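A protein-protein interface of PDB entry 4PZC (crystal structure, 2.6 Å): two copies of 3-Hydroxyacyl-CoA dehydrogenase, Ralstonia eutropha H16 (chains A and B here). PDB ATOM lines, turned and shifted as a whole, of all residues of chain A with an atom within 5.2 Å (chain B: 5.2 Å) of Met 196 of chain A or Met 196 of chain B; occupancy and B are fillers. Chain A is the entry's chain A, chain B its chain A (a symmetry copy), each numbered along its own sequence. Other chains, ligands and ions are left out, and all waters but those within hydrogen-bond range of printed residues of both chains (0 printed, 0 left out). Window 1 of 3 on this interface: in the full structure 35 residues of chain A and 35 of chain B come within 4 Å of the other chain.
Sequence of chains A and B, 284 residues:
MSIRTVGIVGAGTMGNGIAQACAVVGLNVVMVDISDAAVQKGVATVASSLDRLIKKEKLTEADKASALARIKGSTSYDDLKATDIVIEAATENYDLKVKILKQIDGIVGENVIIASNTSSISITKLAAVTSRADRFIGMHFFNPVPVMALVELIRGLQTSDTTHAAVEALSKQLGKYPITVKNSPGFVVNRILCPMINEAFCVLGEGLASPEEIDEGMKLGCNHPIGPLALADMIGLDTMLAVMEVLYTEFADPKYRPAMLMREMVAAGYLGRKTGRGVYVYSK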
ATOM      1  N   ILE A 192      13.943   3.384  10.981  1.00  0.00           N
ATOM      2  CA  ILE A 192      13.766   2.212  11.809  1.00  0.00           C
ATOM      3  C   ILE A 192      14.738   1.064  11.505  1.00  0.00           C
ATOM      4  O   ILE A 192      15.237   0.419  12.434  1.00  0.00           O
ATOM      5  CB  ILE A 192      12.285   1.848  11.978  1.00  0.00           C
ATOM      6  CG1 ILE A 192      11.638   1.371  10.698  1.00  0.00           C
ATOM      7  CG2 ILE A 192      11.571   3.095  12.493  1.00  0.00           C
ATOM      8  CD1 ILE A 192      10.286   2.040  10.409  1.00  0.00           C
ATOM      9  N   LEU A 193      15.069   0.848  10.241  1.00  0.00           N
ATOM     10  CA  LEU A 193      16.059  -0.159   9.925  1.00  0.00           C
ATOM     11  C   LEU A 193      17.366   0.125  10.657  1.00  0.00           C
ATOM     12  O   LEU A 193      17.842  -0.693  11.441  1.00  0.00           O
ATOM     13  CB  LEU A 193      16.285  -0.225   8.423  1.00  0.00           C
ATOM     14  CG  LEU A 193      17.388  -1.191   7.945  1.00  0.00           C
ATOM     15  CD1 LEU A 193      17.052  -2.633   8.267  1.00  0.00           C
ATOM     16  CD2 LEU A 193      17.680  -1.035   6.444  1.00  0.00           C
ATOM     17  N   CYS A 194      17.957   1.285  10.442  1.00  0.00           N
ATOM     18  CA  CYS A 194      19.373   1.402  10.822  1.00  0.00           C
ATOM     19  C   CYS A 194      19.618   1.273  12.303  1.00  0.00           C
ATOM     20  O   CYS A 194      20.639   0.724  12.687  1.00  0.00           O
ATOM     21  CB  CYS A 194      20.006   2.670  10.287  1.00  0.00           C
ATOM     22  SG  CYS A 194      20.259   2.672   8.497  1.00  0.00           S
ATOM     23  N   PRO A 195      18.708   1.789  13.154  1.00  0.00           N
ATOM     24  CA  PRO A 195      18.985   1.589  14.600  1.00  0.00           C
ATOM     25  C   PRO A 195      18.902   0.136  15.015  1.00  0.00           C
ATOM     26  O   PRO A 195      19.541  -0.283  15.999  1.00  0.00           O
ATOM     27  CB  PRO A 195      17.941   2.455  15.297  1.00  0.00           C
ATOM     28  CG  PRO A 195      17.622   3.523  14.301  1.00  0.00           C
ATOM     29  CD  PRO A 195      17.756   2.891  12.926  1.00  0.00           C
ATOM     30  N   MET A 196      18.144  -0.639  14.247  1.00  0.00           N
ATOM     31  CA  MET A 196      18.093  -2.085  14.456  1.00  0.00           C
ATOM     32  C   MET A 196      19.471  -2.672  14.203  1.00  0.00           C
ATOM     33  O   MET A 196      19.951  -3.449  15.015  1.00  0.00           O
ATOM     34  CB  MET A 196      17.105  -2.749  13.525  1.00  0.00           C
ATOM     35  CG  MET A 196      16.897  -4.206  13.844  1.00  0.00           C
ATOM     36  SD  MET A 196      16.224  -5.073  12.417  1.00  0.00           S
ATOM     37  CE  MET A 196      17.761  -5.502  11.605  1.00  0.00           C
ATOM     38  N   ILE A 197      20.089  -2.268  13.090  1.00  0.00           N
ATOM     39  CA  ILE A 197      21.430  -2.708  12.745  1.00  0.00           C
ATOM     40  C   ILE A 197      22.401  -2.331  13.867  1.00  0.00           C
ATOM     41  O   ILE A 197      23.155  -3.169  14.372  1.00  0.00           O
ATOM     42  CB  ILE A 197      21.966  -2.053  11.465  1.00  0.00           C
ATOM     43  CG1 ILE A 197      21.001  -2.212  10.268  1.00  0.00           C
ATOM     44  CG2 ILE A 197      23.345  -2.624  11.157  1.00  0.00           C
ATOM     45  CD1 ILE A 197      20.715  -3.651   9.911  1.00  0.00           C
ATOM     46  N   ASN A 198      22.377  -1.071  14.264  1.00  0.00           N
ATOM     47  CA  ASN A 198      23.068  -0.661  15.476  1.00  0.00           C
ATOM     48  C   ASN A 198      22.889  -1.568  16.704  1.00  0.00           C
ATOM     49  O   ASN A 198      23.874  -1.904  17.412  1.00  0.00           O
ATOM     50  CB  ASN A 198      22.604   0.716  15.897  1.00  0.00           C
ATOM     51  CG  ASN A 198      23.685   1.464  16.579  1.00  0.00           C
ATOM     52  OD1 ASN A 198      23.481   2.070  17.621  1.00  0.00           O
ATOM     53  ND2 ASN A 198      24.884   1.430  15.967  1.00  0.00           N
ATOM     54  N   GLU A 199      21.636  -1.948  16.992  1.00  0.00           N
ATOM     55  CA  GLU A 199      21.415  -2.796  18.167  1.00  0.00           C
ATOM     56  C   GLU A 199      22.201  -4.074  18.023  1.00  0.00           C
ATOM     57  O   GLU A 199      22.735  -4.563  18.993  1.00  0.00           O
ATOM     58  CB  GLU A 199      19.942  -3.123  18.409  1.00  0.00           C
ATOM     59  CG  GLU A 199      19.661  -3.474  19.868  1.00  0.00           C
ATOM     60  CD  GLU A 199      19.870  -2.299  20.823  1.00  0.00           C
ATOM     61  OE1 GLU A 199      19.899  -1.146  20.353  1.00  0.00           O
ATOM     62  OE2 GLU A 199      19.998  -2.526  22.051  1.00  0.00           O
ATOM     63  N   ALA A 200      22.248  -4.617  16.810  1.00  0.00           N
ATOM     64  CA  ALA A 200      23.043  -5.798  16.542  1.00  0.00           C
ATOM     65  C   ALA A 200      24.476  -5.560  16.954  1.00  0.00           C
ATOM     66  O   ALA A 200      25.048  -6.384  17.658  1.00  0.00           O
ATOM     67  CB  ALA A 200      22.991  -6.193  15.083  1.00  0.00           C
ATOM     68  N   HIS A 224      14.071 -12.657   7.934  1.00  0.00           N
ATOM     69  CA  HIS A 224      14.661 -11.572   7.162  1.00  0.00           C
ATOM     70  C   HIS A 224      15.612 -12.220   6.156  1.00  0.00           C
ATOM     71  O   HIS A 224      16.371 -13.117   6.517  1.00  0.00           O
ATOM     72  CB  HIS A 224      15.500 -10.647   8.039  1.00  0.00           C
ATOM     73  CG  HIS A 224      14.727  -9.891   9.068  1.00  0.00           C
ATOM     74  ND1 HIS A 224      15.320  -8.976   9.912  1.00  0.00           N
ATOM     75  CD2 HIS A 224      13.417  -9.901   9.395  1.00  0.00           C
ATOM     76  CE1 HIS A 224      14.414  -8.452  10.715  1.00  0.00           C
ATOM     77  NE2 HIS A 224      13.249  -8.995  10.418  1.00  0.00           N
ATOM     78  N   PRO A 228      21.525  -8.535   9.850  1.00  0.00           N
ATOM     79  CA  PRO A 228      21.944  -7.136   9.950  1.00  0.00           C
ATOM     80  C   PRO A 228      23.446  -6.943   9.931  1.00  0.00           C
ATOM     81  O   PRO A 228      23.904  -5.948   9.393  1.00  0.00           O
ATOM     82  CB  PRO A 228      21.374  -6.688  11.307  1.00  0.00           C
ATOM     83  CG  PRO A 228      21.318  -7.933  12.123  1.00  0.00           C
ATOM     84  CD  PRO A 228      20.989  -9.030  11.137  1.00  0.00           C
ATOM     85  N   ILE B 192      16.985  -7.294  19.429  1.00  0.00           N
ATOM     86  CA  ILE B 192      17.086  -6.354  18.334  1.00  0.00           C
ATOM     87  C   ILE B 192      15.795  -6.179  17.523  1.00  0.00           C
ATOM     88  O   ILE B 192      15.454  -5.052  17.146  1.00  0.00           O
ATOM     89  CB  ILE B 192      18.390  -6.531  17.545  1.00  0.00           C
ATOM     90  CG1 ILE B 192      18.453  -7.836  16.784  1.00  0.00           C
ATOM     91  CG2 ILE B 192      19.538  -6.454  18.548  1.00  0.00           C
ATOM     92  CD1 ILE B 192      19.777  -8.592  16.973  1.00  0.00           C
ATOM     93  N   LEU B 193      15.044  -7.249  17.314  1.00  0.00           N
ATOM     94  CA  LEU B 193      13.771  -7.106  16.640  1.00  0.00           C
ATOM     95  C   LEU B 193      12.883  -6.108  17.376  1.00  0.00           C
ATOM     96  O   LEU B 193      12.471  -5.095  16.817  1.00  0.00           O
ATOM     97  CB  LEU B 193      13.080  -8.455  16.519  1.00  0.00           C
ATOM     98  CG  LEU B 193      11.666  -8.442  15.906  1.00  0.00           C
ATOM     99  CD1 LEU B 193      11.682  -7.976  14.464  1.00  0.00           C
ATOM    100  CD2 LEU B 193      10.976  -9.811  16.016  1.00  0.00           C
ATOM    101  N   CYS B 194      12.592  -6.353  18.640  1.00  0.00           N
ATOM    102  CA  CYS B 194      11.451  -5.631  19.222  1.00  0.00           C
ATOM    103  C   CYS B 194      11.651  -4.139  19.303  1.00  0.00           C
ATOM    104  O   CYS B 194      10.692  -3.405  19.132  1.00  0.00           O
ATOM    105  CB  CYS B 194      11.051  -6.187  20.574  1.00  0.00           C
ATOM    106  SG  CYS B 194      10.266  -7.814  20.502  1.00  0.00           S
ATOM    107  N   PRO B 195      12.884  -3.670  19.581  1.00  0.00           N
ATOM    108  CA  PRO B 195      13.026  -2.191  19.601  1.00  0.00           C
ATOM    109  C   PRO B 195      12.838  -1.568  18.235  1.00  0.00           C
ATOM    110  O   PRO B 195      12.447  -0.391  18.119  1.00  0.00           O
ATOM    111  CB  PRO B 195      14.429  -1.964  20.157  1.00  0.00           C
ATOM    112  CG  PRO B 195      14.699  -3.180  20.984  1.00  0.00           C
ATOM    113  CD  PRO B 195      13.980  -4.335  20.310  1.00  0.00           C
ATOM    114  N   MET B 196      13.080  -2.366  17.200  1.00  0.00           N
ATOM    115  CA  MET B 196      12.801  -1.930  15.833  1.00  0.00           C
ATOM    116  C   MET B 196      11.307  -1.694  15.683  1.00  0.00           C
ATOM    117  O   MET B 196      10.911  -0.661  15.165  1.00  0.00           O
ATOM    118  CB  MET B 196      13.232  -2.964  14.818  1.00  0.00           C
ATOM    119  CG  MET B 196      13.127  -2.465  13.402  1.00  0.00           C
ATOM    120  SD  MET B 196      13.063  -3.848  12.251  1.00  0.00           S
ATOM    121  CE  MET B 196      11.294  -4.126  12.252  1.00  0.00           C
ATOM    122  N   ILE B 197      10.508  -2.652  16.162  1.00  0.00           N
ATOM    123  CA  ILE B 197       9.060  -2.539  16.133  1.00  0.00           C
ATOM    124  C   ILE B 197       8.625  -1.279  16.886  1.00  0.00           C
ATOM    125  O   ILE B 197       7.868  -0.451  16.369  1.00  0.00           O
ATOM    126  CB  ILE B 197       8.352  -3.720  16.810  1.00  0.00           C
ATOM    127  CG1 ILE B 197       8.817  -5.087  16.257  1.00  0.00           C
ATOM    128  CG2 ILE B 197       6.845  -3.539  16.670  1.00  0.00           C
ATOM    129  CD1 ILE B 197       8.578  -5.253  14.776  1.00  0.00           C
ATOM    130  N   ASN B 198       9.111  -1.129  18.105  1.00  0.00           N
ATOM    131  CA  ASN B 198       8.968   0.134  18.812  1.00  0.00           C
ATOM    132  C   ASN B 198       9.266   1.406  18.002  1.00  0.00           C
ATOM    133  O   ASN B 198       8.498   2.401  18.050  1.00  0.00           O
ATOM    134  CB  ASN B 198       9.894   0.168  20.007  1.00  0.00           C
ATOM    135  CG  ASN B 198       9.322   0.976  21.109  1.00  0.00           C
ATOM    136  OD1 ASN B 198       9.995   1.803  21.708  1.00  0.00           O
ATOM    137  ND2 ASN B 198       8.031   0.727  21.397  1.00  0.00           N
ATOM    138  N   GLU B 199      10.395   1.406  17.278  1.00  0.00           N
ATOM    139  CA  GLU B 199      10.731   2.606  16.506  1.00  0.00           C
ATOM    140  C   GLU B 199       9.625   2.905  15.528  1.00  0.00           C
ATOM    141  O   GLU B 199       9.306   4.053  15.313  1.00  0.00           O
ATOM    142  CB  GLU B 199      12.060   2.493  15.761  1.00  0.00           C
ATOM    143  CG  GLU B 199      12.674   3.860  15.465  1.00  0.00           C
ATOM    144  CD  GLU B 199      13.098   4.617  16.724  1.00  0.00           C
ATOM    145  OE1 GLU B 199      13.237   3.979  17.784  1.00  0.00           O
ATOM    146  OE2 GLU B 199      13.300   5.853  16.654  1.00  0.00           O
ATOM    147  N   ALA B 200       9.058   1.863  14.924  1.00  0.00           N
ATOM    148  CA  ALA B 200       7.932   2.029  14.030  1.00  0.00           C
ATOM    149  C   ALA B 200       6.818   2.766  14.735  1.00  0.00           C
ATOM    150  O   ALA B 200       6.292   3.731  14.193  1.00  0.00           O
ATOM    151  CB  ALA B 200       7.419   0.703  13.516  1.00  0.00           C
ATOM    152  N   HIS B 224      11.583  -7.356   4.019  1.00  0.00           N
ATOM    153  CA  HIS B 224      11.100  -8.116   5.164  1.00  0.00           C
ATOM    154  C   HIS B 224       9.746  -8.698   4.760  1.00  0.00           C
ATOM    155  O   HIS B 224       8.923  -7.996   4.177  1.00  0.00           O
ATOM    156  CB  HIS B 224      10.857  -7.219   6.376  1.00  0.00           C
ATOM    157  CG  HIS B 224      12.086  -6.586   6.939  1.00  0.00           C
ATOM    158  ND1 HIS B 224      12.054  -5.785   8.061  1.00  0.00           N
ATOM    159  CD2 HIS B 224      13.378  -6.629   6.551  1.00  0.00           C
ATOM    160  CE1 HIS B 224      13.271  -5.361   8.345  1.00  0.00           C
ATOM    161  NE2 HIS B 224      14.094  -5.863   7.444  1.00  0.00           N
ATOM    162  N   PRO B 228       6.499  -4.241  10.397  1.00  0.00           N
ATOM    163  CA  PRO B 228       6.527  -4.277  11.861  1.00  0.00           C
ATOM    164  C   PRO B 228       5.204  -3.922  12.507  1.00  0.00           C
ATOM    165  O   PRO B 228       4.889  -4.481  13.546  1.00  0.00           O
ATOM    166  CB  PRO B 228       7.589  -3.224  12.224  1.00  0.00           C
ATOM    167  CG  PRO B 228       7.556  -2.250  11.098  1.00  0.00           C
ATOM    168  CD  PRO B 228       7.253  -3.082   9.873  1.00  0.00           C
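Among the printed residues, merely in contact across the chains: Ile 192 of chain A with Met 196 of chain B (3.7 Å), Ile 192 of chain A with Glu 199 of chain B (3.3 Å), Ile 192 of chain A with Ala 200 of chain B (3.7 Å), Met 196 of chain A with Ile 192 of chain B (3.7 Å), Glu 199 of chain A with Ile 192 of chain B (3.3 Å) and Ala 200 of chain A with Ile 192 of chain B (3.7 Å).
SD of Met 196 of chain B lies close to SD of Met 196 of chain A (3.4 Å).
Ile 192 of chain A touches Met 196 of chain B, and with the chains exchanged Met 196 of chain A touches Ile 192 of chain B. Ile 192 of chain A touches Glu 199 of chain B, and with the chains exchanged Glu 199 of chain A touches Ile 192 of chain B. Ile 192 of chain A touches Ala 200 of chain B, and with the chains exchanged Ala 200 of chain A touches Ile 192 of chain B. Met 196 of chain B touches its own counterpart, Met 196 of chain A. Of the 7 pairs that touch across the chains among the printed residues, 7 have their exchanged pair printed and touching as well.
Of the 11 printed residues of chain B, 4 touch a printed residue of chain A. Hydrophobic or aromatic side chains of chain B within 4 Å of the printed part of chain A: Ile 192 and Met 196. Of the 11 printed residues of chain A, 4 touch a printed residue of chain B. Printed residues of chain A that touch a printed residue of chain B: Ile 192, Met 196, Glu 199 and Ala 200. Hydrophobic or aromatic side chains of chain A that line the printed part of chain B: Ile 192 and Met 196.
Of the printed residues of chain B, Ile 192 of chain A touches Met 196, Glu 199 and Ala 200. Leu 193 of chain A touches none of the printed residues of chain B. Printed residues of chain B within 4 Å of Glu 199 of chain A: Ile 192. His 224 of chain A touches none of the printed residues of chain B. Of the printed residues of chain A, Ala 200 of chain B touches Ile 192 (3.7 Å). The nearest residue of chain B that does not touch Met 196 of chain A is Leu 193 of chain B (5.0 Å). The nearest printed residue of chain B that does not touch Glu 199 of chain A is Pro 195 of chain B (5.1 Å).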
